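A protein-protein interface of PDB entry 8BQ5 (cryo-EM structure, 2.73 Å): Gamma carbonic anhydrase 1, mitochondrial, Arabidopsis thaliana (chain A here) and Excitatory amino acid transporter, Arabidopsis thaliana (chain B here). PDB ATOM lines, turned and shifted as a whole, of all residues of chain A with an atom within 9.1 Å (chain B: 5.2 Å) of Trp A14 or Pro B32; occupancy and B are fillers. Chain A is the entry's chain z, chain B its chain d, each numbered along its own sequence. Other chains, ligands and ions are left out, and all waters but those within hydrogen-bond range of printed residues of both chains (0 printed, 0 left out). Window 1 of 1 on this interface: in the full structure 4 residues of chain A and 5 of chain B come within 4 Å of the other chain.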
ATOM      1  N   ARG A   6       1.422 -13.571   5.491  1.00  0.00           N
ATOM      2  CA  ARG A   6       2.117 -13.669   4.183  1.00  0.00           C
ATOM      3  C   ARG A   6       1.655 -12.523   3.271  1.00  0.00           C
ATOM      4  O   ARG A   6       2.509 -11.982   2.551  1.00  0.00           O
ATOM      5  CB  ARG A   6       1.916 -15.064   3.583  1.00  0.00           C
ATOM      6  CG  ARG A   6       2.607 -15.291   2.246  1.00  0.00           C
ATOM      7  CD  ARG A   6       2.420 -16.716   1.757  1.00  0.00           C
ATOM      8  NE  ARG A   6       3.066 -17.038   0.493  1.00  0.00           N
ATOM      9  CZ  ARG A   6       3.180 -18.267  -0.002  1.00  0.00           C
ATOM     10  NH1 ARG A   6       2.681 -19.300   0.657  1.00  0.00           N
ATOM     11  NH2 ARG A   6       3.788 -18.460  -1.160  1.00  0.00           N
ATOM     12  N   ALA A   7       0.374 -12.144   3.315  1.00  0.00           N
ATOM     13  CA  ALA A   7      -0.106 -11.013   2.526  1.00  0.00           C
ATOM     14  C   ALA A   7       0.531  -9.709   2.990  1.00  0.00           C
ATOM     15  O   ALA A   7       0.944  -8.875   2.172  1.00  0.00           O
ATOM     16  CB  ALA A   7      -1.630 -10.927   2.610  1.00  0.00           C
ATOM     17  N   PHE A   8       0.614  -9.516   4.308  1.00  0.00           N
ATOM     18  CA  PHE A   8       1.256  -8.315   4.831  1.00  0.00           C
ATOM     19  C   PHE A   8       2.735  -8.284   4.469  1.00  0.00           C
ATOM     20  O   PHE A   8       3.281  -7.223   4.153  1.00  0.00           O
ATOM     21  CB  PHE A   8       1.063  -8.236   6.343  1.00  0.00           C
ATOM     22  CG  PHE A   8      -0.161  -7.475   6.757  1.00  0.00           C
ATOM     23  CD1 PHE A   8      -1.369  -8.124   6.948  1.00  0.00           C
ATOM     24  CD2 PHE A   8      -0.104  -6.106   6.953  1.00  0.00           C
ATOM     25  CE1 PHE A   8      -2.495  -7.424   7.330  1.00  0.00           C
ATOM     26  CE2 PHE A   8      -1.228  -5.399   7.334  1.00  0.00           C
ATOM     27  CZ  PHE A   8      -2.424  -6.059   7.522  1.00  0.00           C
ATOM     28  N   TYR A   9       3.393  -9.440   4.541  1.00  0.00           N
ATOM     29  CA  TYR A   9       4.836  -9.550   4.210  1.00  0.00           C
ATOM     30  C   TYR A   9       5.040  -9.178   2.736  1.00  0.00           C
ATOM     31  O   TYR A   9       5.989  -8.444   2.439  1.00  0.00           O
ATOM     32  CB  TYR A   9       5.292 -10.969   4.554  1.00  0.00           C
ATOM     33  CG  TYR A   9       6.778 -11.210   4.606  1.00  0.00           C
ATOM     34  CD1 TYR A   9       7.519 -10.855   5.720  1.00  0.00           C
ATOM     35  CD2 TYR A   9       7.435 -11.840   3.563  1.00  0.00           C
ATOM     36  CE1 TYR A   9       8.882 -11.088   5.781  1.00  0.00           C
ATOM     37  CE2 TYR A   9       8.796 -12.087   3.611  1.00  0.00           C
ATOM     38  CZ  TYR A   9       9.521 -11.707   4.724  1.00  0.00           C
ATOM     39  OH  TYR A   9      10.861 -11.947   4.776  1.00  0.00           O
ATOM     40  N   SER A  10       4.145  -9.634   1.859  1.00  0.00           N
ATOM     41  CA  SER A  10       4.218  -9.325   0.407  1.00  0.00           C
ATOM     42  C   SER A  10       3.985  -7.835   0.160  1.00  0.00           C
ATOM     43  O   SER A  10       4.763  -7.243  -0.602  1.00  0.00           O
ATOM     44  CB  SER A  10       3.233 -10.158  -0.357  1.00  0.00           C
ATOM     45  OG  SER A  10       3.558 -11.534  -0.248  1.00  0.00           O
ATOM     46  N   VAL A  11       2.965  -7.252   0.786  1.00  0.00           N
ATOM     47  CA  VAL A  11       2.622  -5.821   0.554  1.00  0.00           C
ATOM     48  C   VAL A  11       3.761  -4.965   1.107  1.00  0.00           C
ATOM     49  O   VAL A  11       4.076  -3.949   0.476  1.00  0.00           O
ATOM     50  CB  VAL A  11       1.240  -5.469   1.144  1.00  0.00           C
ATOM     51  CG1 VAL A  11       0.944  -3.980   1.063  1.00  0.00           C
ATOM     52  CG2 VAL A  11       0.134  -6.258   0.463  1.00  0.00           C
ATOM     53  N   GLY A  12       4.373  -5.384   2.220  1.00  0.00           N
ATOM     54  CA  GLY A  12       5.542  -4.668   2.760  1.00  0.00           C
ATOM     55  C   GLY A  12       6.674  -4.628   1.750  1.00  0.00           C
ATOM     56  O   GLY A  12       7.293  -3.581   1.637  1.00  0.00           O
ATOM     57  N   PHE A  13       6.904  -5.723   1.019  1.00  0.00           N
ATOM     58  CA  PHE A  13       7.965  -5.769  -0.025  1.00  0.00           C
ATOM     59  C   PHE A  13       7.664  -4.745  -1.128  1.00  0.00           C
ATOM     60  O   PHE A  13       8.618  -4.149  -1.619  1.00  0.00           O
ATOM     61  CB  PHE A  13       8.111  -7.174  -0.615  1.00  0.00           C
ATOM     62  CG  PHE A  13       9.157  -8.060   0.008  1.00  0.00           C
ATOM     63  CD1 PHE A  13      10.398  -7.558   0.362  1.00  0.00           C
ATOM     64  CD2 PHE A  13       8.912  -9.409   0.207  1.00  0.00           C
ATOM     65  CE1 PHE A  13      11.361  -8.381   0.922  1.00  0.00           C
ATOM     66  CE2 PHE A  13       9.877 -10.230   0.766  1.00  0.00           C
ATOM     67  CZ  PHE A  13      11.099  -9.715   1.123  1.00  0.00           C
ATOM     68  N   TRP A  14       6.388  -4.560  -1.496  1.00  0.00           N
ATOM     69  CA  TRP A  14       5.997  -3.536  -2.507  1.00  0.00           C
ATOM     70  C   TRP A  14       6.363  -2.142  -1.998  1.00  0.00           C
ATOM     71  O   TRP A  14       6.964  -1.372  -2.770  1.00  0.00           O
ATOM     72  CB  TRP A  14       4.498  -3.604  -2.852  1.00  0.00           C
ATOM     73  CG  TRP A  14       3.961  -4.948  -3.231  1.00  0.00           C
ATOM     74  CD1 TRP A  14       4.660  -6.074  -3.555  1.00  0.00           C
ATOM     75  CD2 TRP A  14       2.572  -5.297  -3.346  1.00  0.00           C
ATOM     76  NE1 TRP A  14       3.804  -7.099  -3.848  1.00  0.00           N
ATOM     77  CE2 TRP A  14       2.515  -6.652  -3.730  1.00  0.00           C
ATOM     78  CE3 TRP A  14       1.375  -4.598  -3.158  1.00  0.00           C
ATOM     79  CZ2 TRP A  14       1.307  -7.317  -3.926  1.00  0.00           C
ATOM     80  CZ3 TRP A  14       0.182  -5.257  -3.351  1.00  0.00           C
ATOM     81  CH2 TRP A  14       0.151  -6.597  -3.731  1.00  0.00           C
ATOM     82  N   ILE A  15       6.020  -1.833  -0.747  1.00  0.00           N
ATOM     83  CA  ILE A  15       6.350  -0.500  -0.156  1.00  0.00           C
ATOM     84  C   ILE A  15       7.870  -0.355  -0.057  1.00  0.00           C
ATOM     85  O   ILE A  15       8.374   0.734  -0.355  1.00  0.00           O
ATOM     86  CB  ILE A  15       5.668  -0.307   1.216  1.00  0.00           C
ATOM     87  CG1 ILE A  15       4.185  -0.678   1.167  1.00  0.00           C
ATOM     88  CG2 ILE A  15       5.878   1.102   1.742  1.00  0.00           C
ATOM     89  CD1 ILE A  15       3.523  -0.721   2.520  1.00  0.00           C
ATOM     90  N   ARG A  16       8.562  -1.411   0.369  1.00  0.00           N
ATOM     91  CA  ARG A  16      10.039  -1.361   0.517  1.00  0.00           C
ATOM     92  C   ARG A  16      10.702  -1.165  -0.851  1.00  0.00           C
ATOM     93  O   ARG A  16      11.546  -0.277  -0.954  1.00  0.00           O
ATOM     94  CB  ARG A  16      10.574  -2.635   1.166  1.00  0.00           C
ATOM     95  CG  ARG A  16      10.165  -2.815   2.619  1.00  0.00           C
ATOM     96  CD  ARG A  16      10.906  -3.972   3.252  1.00  0.00           C
ATOM     97  NE  ARG A  16      12.319  -3.656   3.376  1.00  0.00           N
ATOM     98  CZ  ARG A  16      13.220  -4.429   3.964  1.00  0.00           C
ATOM     99  NH1 ARG A  16      12.859  -5.582   4.500  1.00  0.00           N
ATOM    100  NH2 ARG A  16      14.481  -4.043   4.022  1.00  0.00           N
ATOM    101  N   GLU A  17      10.313  -1.963  -1.846  1.00  0.00           N
ATOM    102  CA  GLU A  17      10.885  -1.822  -3.210  1.00  0.00           C
ATOM    103  C   GLU A  17      10.632  -0.404  -3.732  1.00  0.00           C
ATOM    104  O   GLU A  17      11.545   0.158  -4.355  1.00  0.00           O
ATOM    105  CB  GLU A  17      10.330  -2.873  -4.166  1.00  0.00           C
ATOM    106  CG  GLU A  17      10.953  -2.778  -5.543  1.00  0.00           C
ATOM    107  CD  GLU A  17      10.685  -3.938  -6.480  1.00  0.00           C
ATOM    108  OE1 GLU A  17       9.764  -4.727  -6.200  1.00  0.00           O
ATOM    109  OE2 GLU A  17      11.403  -4.046  -7.491  1.00  0.00           O
ATOM    110  N   THR A  18       9.450   0.156  -3.468  1.00  0.00           N
ATOM    111  CA  THR A  18       9.196   1.531  -3.889  1.00  0.00           C
ATOM    112  C   THR A  18      10.121   2.510  -3.170  1.00  0.00           C
ATOM    113  O   THR A  18      10.683   3.418  -3.796  1.00  0.00           O
ATOM    114  CB  THR A  18       7.732   1.888  -3.640  1.00  0.00           C
ATOM    115  OG1 THR A  18       6.889   0.986  -4.367  1.00  0.00           O
ATOM    116  CG2 THR A  18       7.447   3.307  -4.086  1.00  0.00           C
ATOM    117  N   GLY A  19      10.303   2.333  -1.860  1.00  0.00           N
ATOM    118  CA  GLY A  19      11.185   3.227  -1.121  1.00  0.00           C
ATOM    119  C   GLY A  19      12.633   3.130  -1.563  1.00  0.00           C
ATOM    120  O   GLY A  19      13.335   4.140  -1.664  1.00  0.00           O
ATOM    121  N   GLN A  20      13.104   1.910  -1.825  1.00  0.00           N
ATOM    122  CA  GLN A  20      14.482   1.719  -2.269  1.00  0.00           C
ATOM    123  C   GLN A  20      14.706   2.335  -3.645  1.00  0.00           C
ATOM    124  O   GLN A  20      15.748   2.956  -3.895  1.00  0.00           O
ATOM    125  CB  GLN A  20      14.815   0.229  -2.274  1.00  0.00           C
ATOM    126  CG  GLN A  20      14.768  -0.393  -0.891  1.00  0.00           C
ATOM    127  CD  GLN A  20      15.364  -1.779  -0.839  1.00  0.00           C
ATOM    128  OE1 GLN A  20      16.210  -2.138  -1.656  1.00  0.00           O
ATOM    129  NE2 GLN A  20      14.905  -2.580   0.114  1.00  0.00           N
ATOM    130  N   ALA A  21      13.732   2.185  -4.547  1.00  0.00           N
ATOM    131  CA  ALA A  21      13.817   2.850  -5.843  1.00  0.00           C
ATOM    132  C   ALA A  21      13.843   4.365  -5.685  1.00  0.00           C
ATOM    133  O   ALA A  21      14.568   5.062  -6.405  1.00  0.00           O
ATOM    134  CB  ALA A  21      12.648   2.424  -6.728  1.00  0.00           C
ATOM    135  N   LEU A  22      13.047   4.893  -4.751  1.00  0.00           N
ATOM    136  CA  LEU A  22      13.067   6.328  -4.487  1.00  0.00           C
ATOM    137  C   LEU A  22      14.443   6.779  -4.011  1.00  0.00           C
ATOM    138  O   LEU A  22      14.945   7.833  -4.426  1.00  0.00           O
ATOM    139  CB  LEU A  22      12.002   6.674  -3.449  1.00  0.00           C
ATOM    140  CG  LEU A  22      10.692   7.271  -3.958  1.00  0.00           C
ATOM    141  CD1 LEU A  22       9.828   7.709  -2.791  1.00  0.00           C
ATOM    142  CD2 LEU A  22      10.959   8.432  -4.896  1.00  0.00           C
ATOM    143  N   MET B  29       4.256  -8.114  -9.459  1.00  0.00           N
ATOM    144  CA  MET B  29       4.402  -6.789  -8.868  1.00  0.00           C
ATOM    145  C   MET B  29       5.855  -6.326  -8.845  1.00  0.00           C
ATOM    146  O   MET B  29       6.358  -5.879  -7.813  1.00  0.00           O
ATOM    147  CB  MET B  29       3.823  -6.777  -7.458  1.00  0.00           C
ATOM    148  CG  MET B  29       2.482  -7.471  -7.354  1.00  0.00           C
ATOM    149  SD  MET B  29       1.259  -6.696  -8.423  1.00  0.00           S
ATOM    150  CE  MET B  29       1.043  -5.133  -7.579  1.00  0.00           C
ATOM    151  N   ARG B  30       6.542  -6.398  -9.986  1.00  0.00           N
ATOM    152  CA  ARG B  30       7.964  -6.071 -10.002  1.00  0.00           C
ATOM    153  C   ARG B  30       8.192  -4.585  -9.738  1.00  0.00           C
ATOM    154  O   ARG B  30       9.001  -4.220  -8.882  1.00  0.00           O
ATOM    155  CB  ARG B  30       8.591  -6.518 -11.327  1.00  0.00           C
ATOM    156  CG  ARG B  30       9.932  -5.874 -11.712  1.00  0.00           C
ATOM    157  CD  ARG B  30      11.005  -5.865 -10.613  1.00  0.00           C
ATOM    158  NE  ARG B  30      11.135  -7.122  -9.887  1.00  0.00           N
ATOM    159  CZ  ARG B  30      12.173  -7.942  -9.990  1.00  0.00           C
ATOM    160  NH1 ARG B  30      13.180  -7.683 -10.807  1.00  0.00           N
ATOM    161  NH2 ARG B  30      12.201  -9.048  -9.253  1.00  0.00           N
ATOM    162  N   HIS B  31       7.475  -3.710 -10.437  1.00  0.00           N
ATOM    163  CA  HIS B  31       7.603  -2.266 -10.232  1.00  0.00           C
ATOM    164  C   HIS B  31       6.220  -1.699  -9.939  1.00  0.00           C
ATOM    165  O   HIS B  31       5.530  -1.219 -10.851  1.00  0.00           O
ATOM    166  CB  HIS B  31       8.237  -1.590 -11.445  1.00  0.00           C
ATOM    167  CG  HIS B  31       9.724  -1.752 -11.526  1.00  0.00           C
ATOM    168  ND1 HIS B  31      10.458  -1.335 -12.615  1.00  0.00           N
ATOM    169  CD2 HIS B  31      10.614  -2.280 -10.653  1.00  0.00           C
ATOM    170  CE1 HIS B  31      11.736  -1.602 -12.411  1.00  0.00           C
ATOM    171  NE2 HIS B  31      11.857  -2.174 -11.229  1.00  0.00           N
ATOM    172  N   PRO B  32       5.775  -1.737  -8.678  1.00  0.00           N
ATOM    173  CA  PRO B  32       4.371  -1.390  -8.375  1.00  0.00           C
ATOM    174  C   PRO B  32       3.966   0.036  -8.739  1.00  0.00           C
ATOM    175  O   PRO B  32       2.784   0.278  -9.039  1.00  0.00           O
ATOM    176  CB  PRO B  32       4.269  -1.644  -6.863  1.00  0.00           C
ATOM    177  CG  PRO B  32       5.681  -1.711  -6.366  1.00  0.00           C
ATOM    178  CD  PRO B  32       6.502  -2.225  -7.496  1.00  0.00           C
ATOM    179  N   TRP B  33       4.897   0.994  -8.717  1.00  0.00           N
ATOM    180  CA  TRP B  33       4.552   2.331  -9.189  1.00  0.00           C
ATOM    181  C   TRP B  33       4.107   2.297 -10.644  1.00  0.00           C
ATOM    182  O   TRP B  33       3.244   3.084 -11.052  1.00  0.00           O
ATOM    183  CB  TRP B  33       5.728   3.295  -9.015  1.00  0.00           C
ATOM    184  CG  TRP B  33       6.998   2.837  -9.655  1.00  0.00           C
ATOM    185  CD1 TRP B  33       7.445   3.151 -10.903  1.00  0.00           C
ATOM    186  CD2 TRP B  33       8.011   2.022  -9.059  1.00  0.00           C
ATOM    187  NE1 TRP B  33       8.661   2.557 -11.134  1.00  0.00           N
ATOM    188  CE2 TRP B  33       9.033   1.862 -10.015  1.00  0.00           C
ATOM    189  CE3 TRP B  33       8.150   1.403  -7.814  1.00  0.00           C
ATOM    190  CZ2 TRP B  33      10.174   1.109  -9.765  1.00  0.00           C
ATOM    191  CZ3 TRP B  33       9.284   0.656  -7.568  1.00  0.00           C
ATOM    192  CH2 TRP B  33      10.281   0.515  -8.540  1.00  0.00           C
ATOM    193  N   GLU B  34       4.670   1.383 -11.436  1.00  0.00           N
ATOM    194  CA  GLU B  34       4.208   1.215 -12.806  1.00  0.00           C
ATOM    195  C   GLU B  34       2.789   0.667 -12.854  1.00  0.00           C
ATOM    196  O   GLU B  34       2.037   0.993 -13.774  1.00  0.00           O
ATOM    197  CB  GLU B  34       5.159   0.304 -13.574  1.00  0.00           C
ATOM    198  CG  GLU B  34       6.573   0.830 -13.620  1.00  0.00           C
ATOM    199  CD  GLU B  34       7.521  -0.117 -14.312  1.00  0.00           C
ATOM    200  OE1 GLU B  34       7.100  -1.239 -14.659  1.00  0.00           O
ATOM    201  OE2 GLU B  34       8.693   0.259 -14.499  1.00  0.00           O
ATOM    202  N   HIS B  35       2.401  -0.155 -11.876  1.00  0.00           N
ATOM    203  CA  HIS B  35       1.007  -0.578 -11.790  1.00  0.00           C
ATOM    204  C   HIS B  35       0.096   0.610 -11.514  1.00  0.00           C
ATOM    205  O   HIS B  35      -0.999   0.711 -12.080  1.00  0.00           O
ATOM    206  CB  HIS B  35       0.839  -1.641 -10.705  1.00  0.00           C
ATOM    207  CG  HIS B  35       1.581  -2.911 -10.979  1.00  0.00           C
ATOM    208  ND1 HIS B  35       2.957  -2.979 -11.001  1.00  0.00           N
ATOM    209  CD2 HIS B  35       1.138  -4.164 -11.236  1.00  0.00           C
ATOM    210  CE1 HIS B  35       3.330  -4.218 -11.262  1.00  0.00           C
ATOM    211  NE2 HIS B  35       2.246  -4.957 -11.409  1.00  0.00           N
ATOM    212  N   VAL B  36       0.531   1.521 -10.639  1.00  0.00           N
ATOM    213  CA  VAL B  36      -0.259   2.724 -10.367  1.00  0.00           C
ATOM    214  C   VAL B  36      -0.406   3.561 -11.637  1.00  0.00           C
ATOM    215  O   VAL B  36      -1.504   4.029 -11.983  1.00  0.00           O
ATOM    216  CB  VAL B  36       0.382   3.530  -9.222  1.00  0.00           C
ATOM    217  CG1 VAL B  36      -0.390   4.811  -8.962  1.00  0.00           C
ATOM    218  CG2 VAL B  36       0.460   2.679  -7.963  1.00  0.00           C
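The guanidinium group (NE) of Arg B30 is in salt-bridge range of the side-chain carboxylate (OE2) of Glu A17, 3.9 Å away.
A ring nitrogen (ND1) of His B35 lies within hydrogen-bond range of the backbone carbonyl oxygen of His B31 (3.1 Å). The side-chain hydroxyl (OG1) of Thr A18 sits at hydrogen-bond distance from the backbone carbonyl oxygen (O) of Trp A14, 2.8 Å away. The indole nitrogen (NE1) of Trp A14 sits close to the backbone carbonyl oxygen (O) of Ser A10 (3.4 Å). A ring nitrogen (NE2) of His B35 lies within hydrogen-bond range of the side-chain sulfur (SD) of Met B29. OE2 of Glu B34 lies within hydrogen-bond range of ND1 of His B31 (3.0 Å).
Among the printed residues, pairs that only touch across the chains: Ala A21 with Trp B33, Thr A18 with Pro B32, Trp A14 with Met B29, Thr A18 with Trp B33, Glu A17 with His B31, Trp A14 with Pro B32, Glu A17 with Met B29 and Glu A17 with Trp B33.
Phe A13 touches none of the printed residues of chain B. Of chain B, only Met B29 (3.6 Å) and Pro B32 (3.8 Å) come within 4 Å of Trp A14. Of the printed residues of chain B, Thr A18 touches Pro B32 and Trp B33. Leu A22 touches none of the printed residues of chain B. Of the printed residues of chain A, Arg B30 touches Glu A17. Of the printed residues of chain A, His B31 touches Glu A17 (3.7 Å). Pro B32 touches just these residues of chain A: Trp A14 (3.8 Å) and Thr A18 (3.6 Å). The nearest printed residue of chain B that does not touch Trp A14 is Trp B33 (5.7 Å).
Hydrophobic or aromatic side chains of chain B that line the printed part of chain A: Met B29, His B31, Pro B32 and Trp B33. Printed residues of chain A that touch a printed residue of chain B: Trp A14, Glu A17, Thr A18 and Ala A21. Among the printed residues, 9 pairs touch across the chains. Among the printed residues, Asp or Glu carboxylates within 4 Å of a Lys or Arg side-chain nitrogen of the other chain: Glu A17 with Arg B30.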
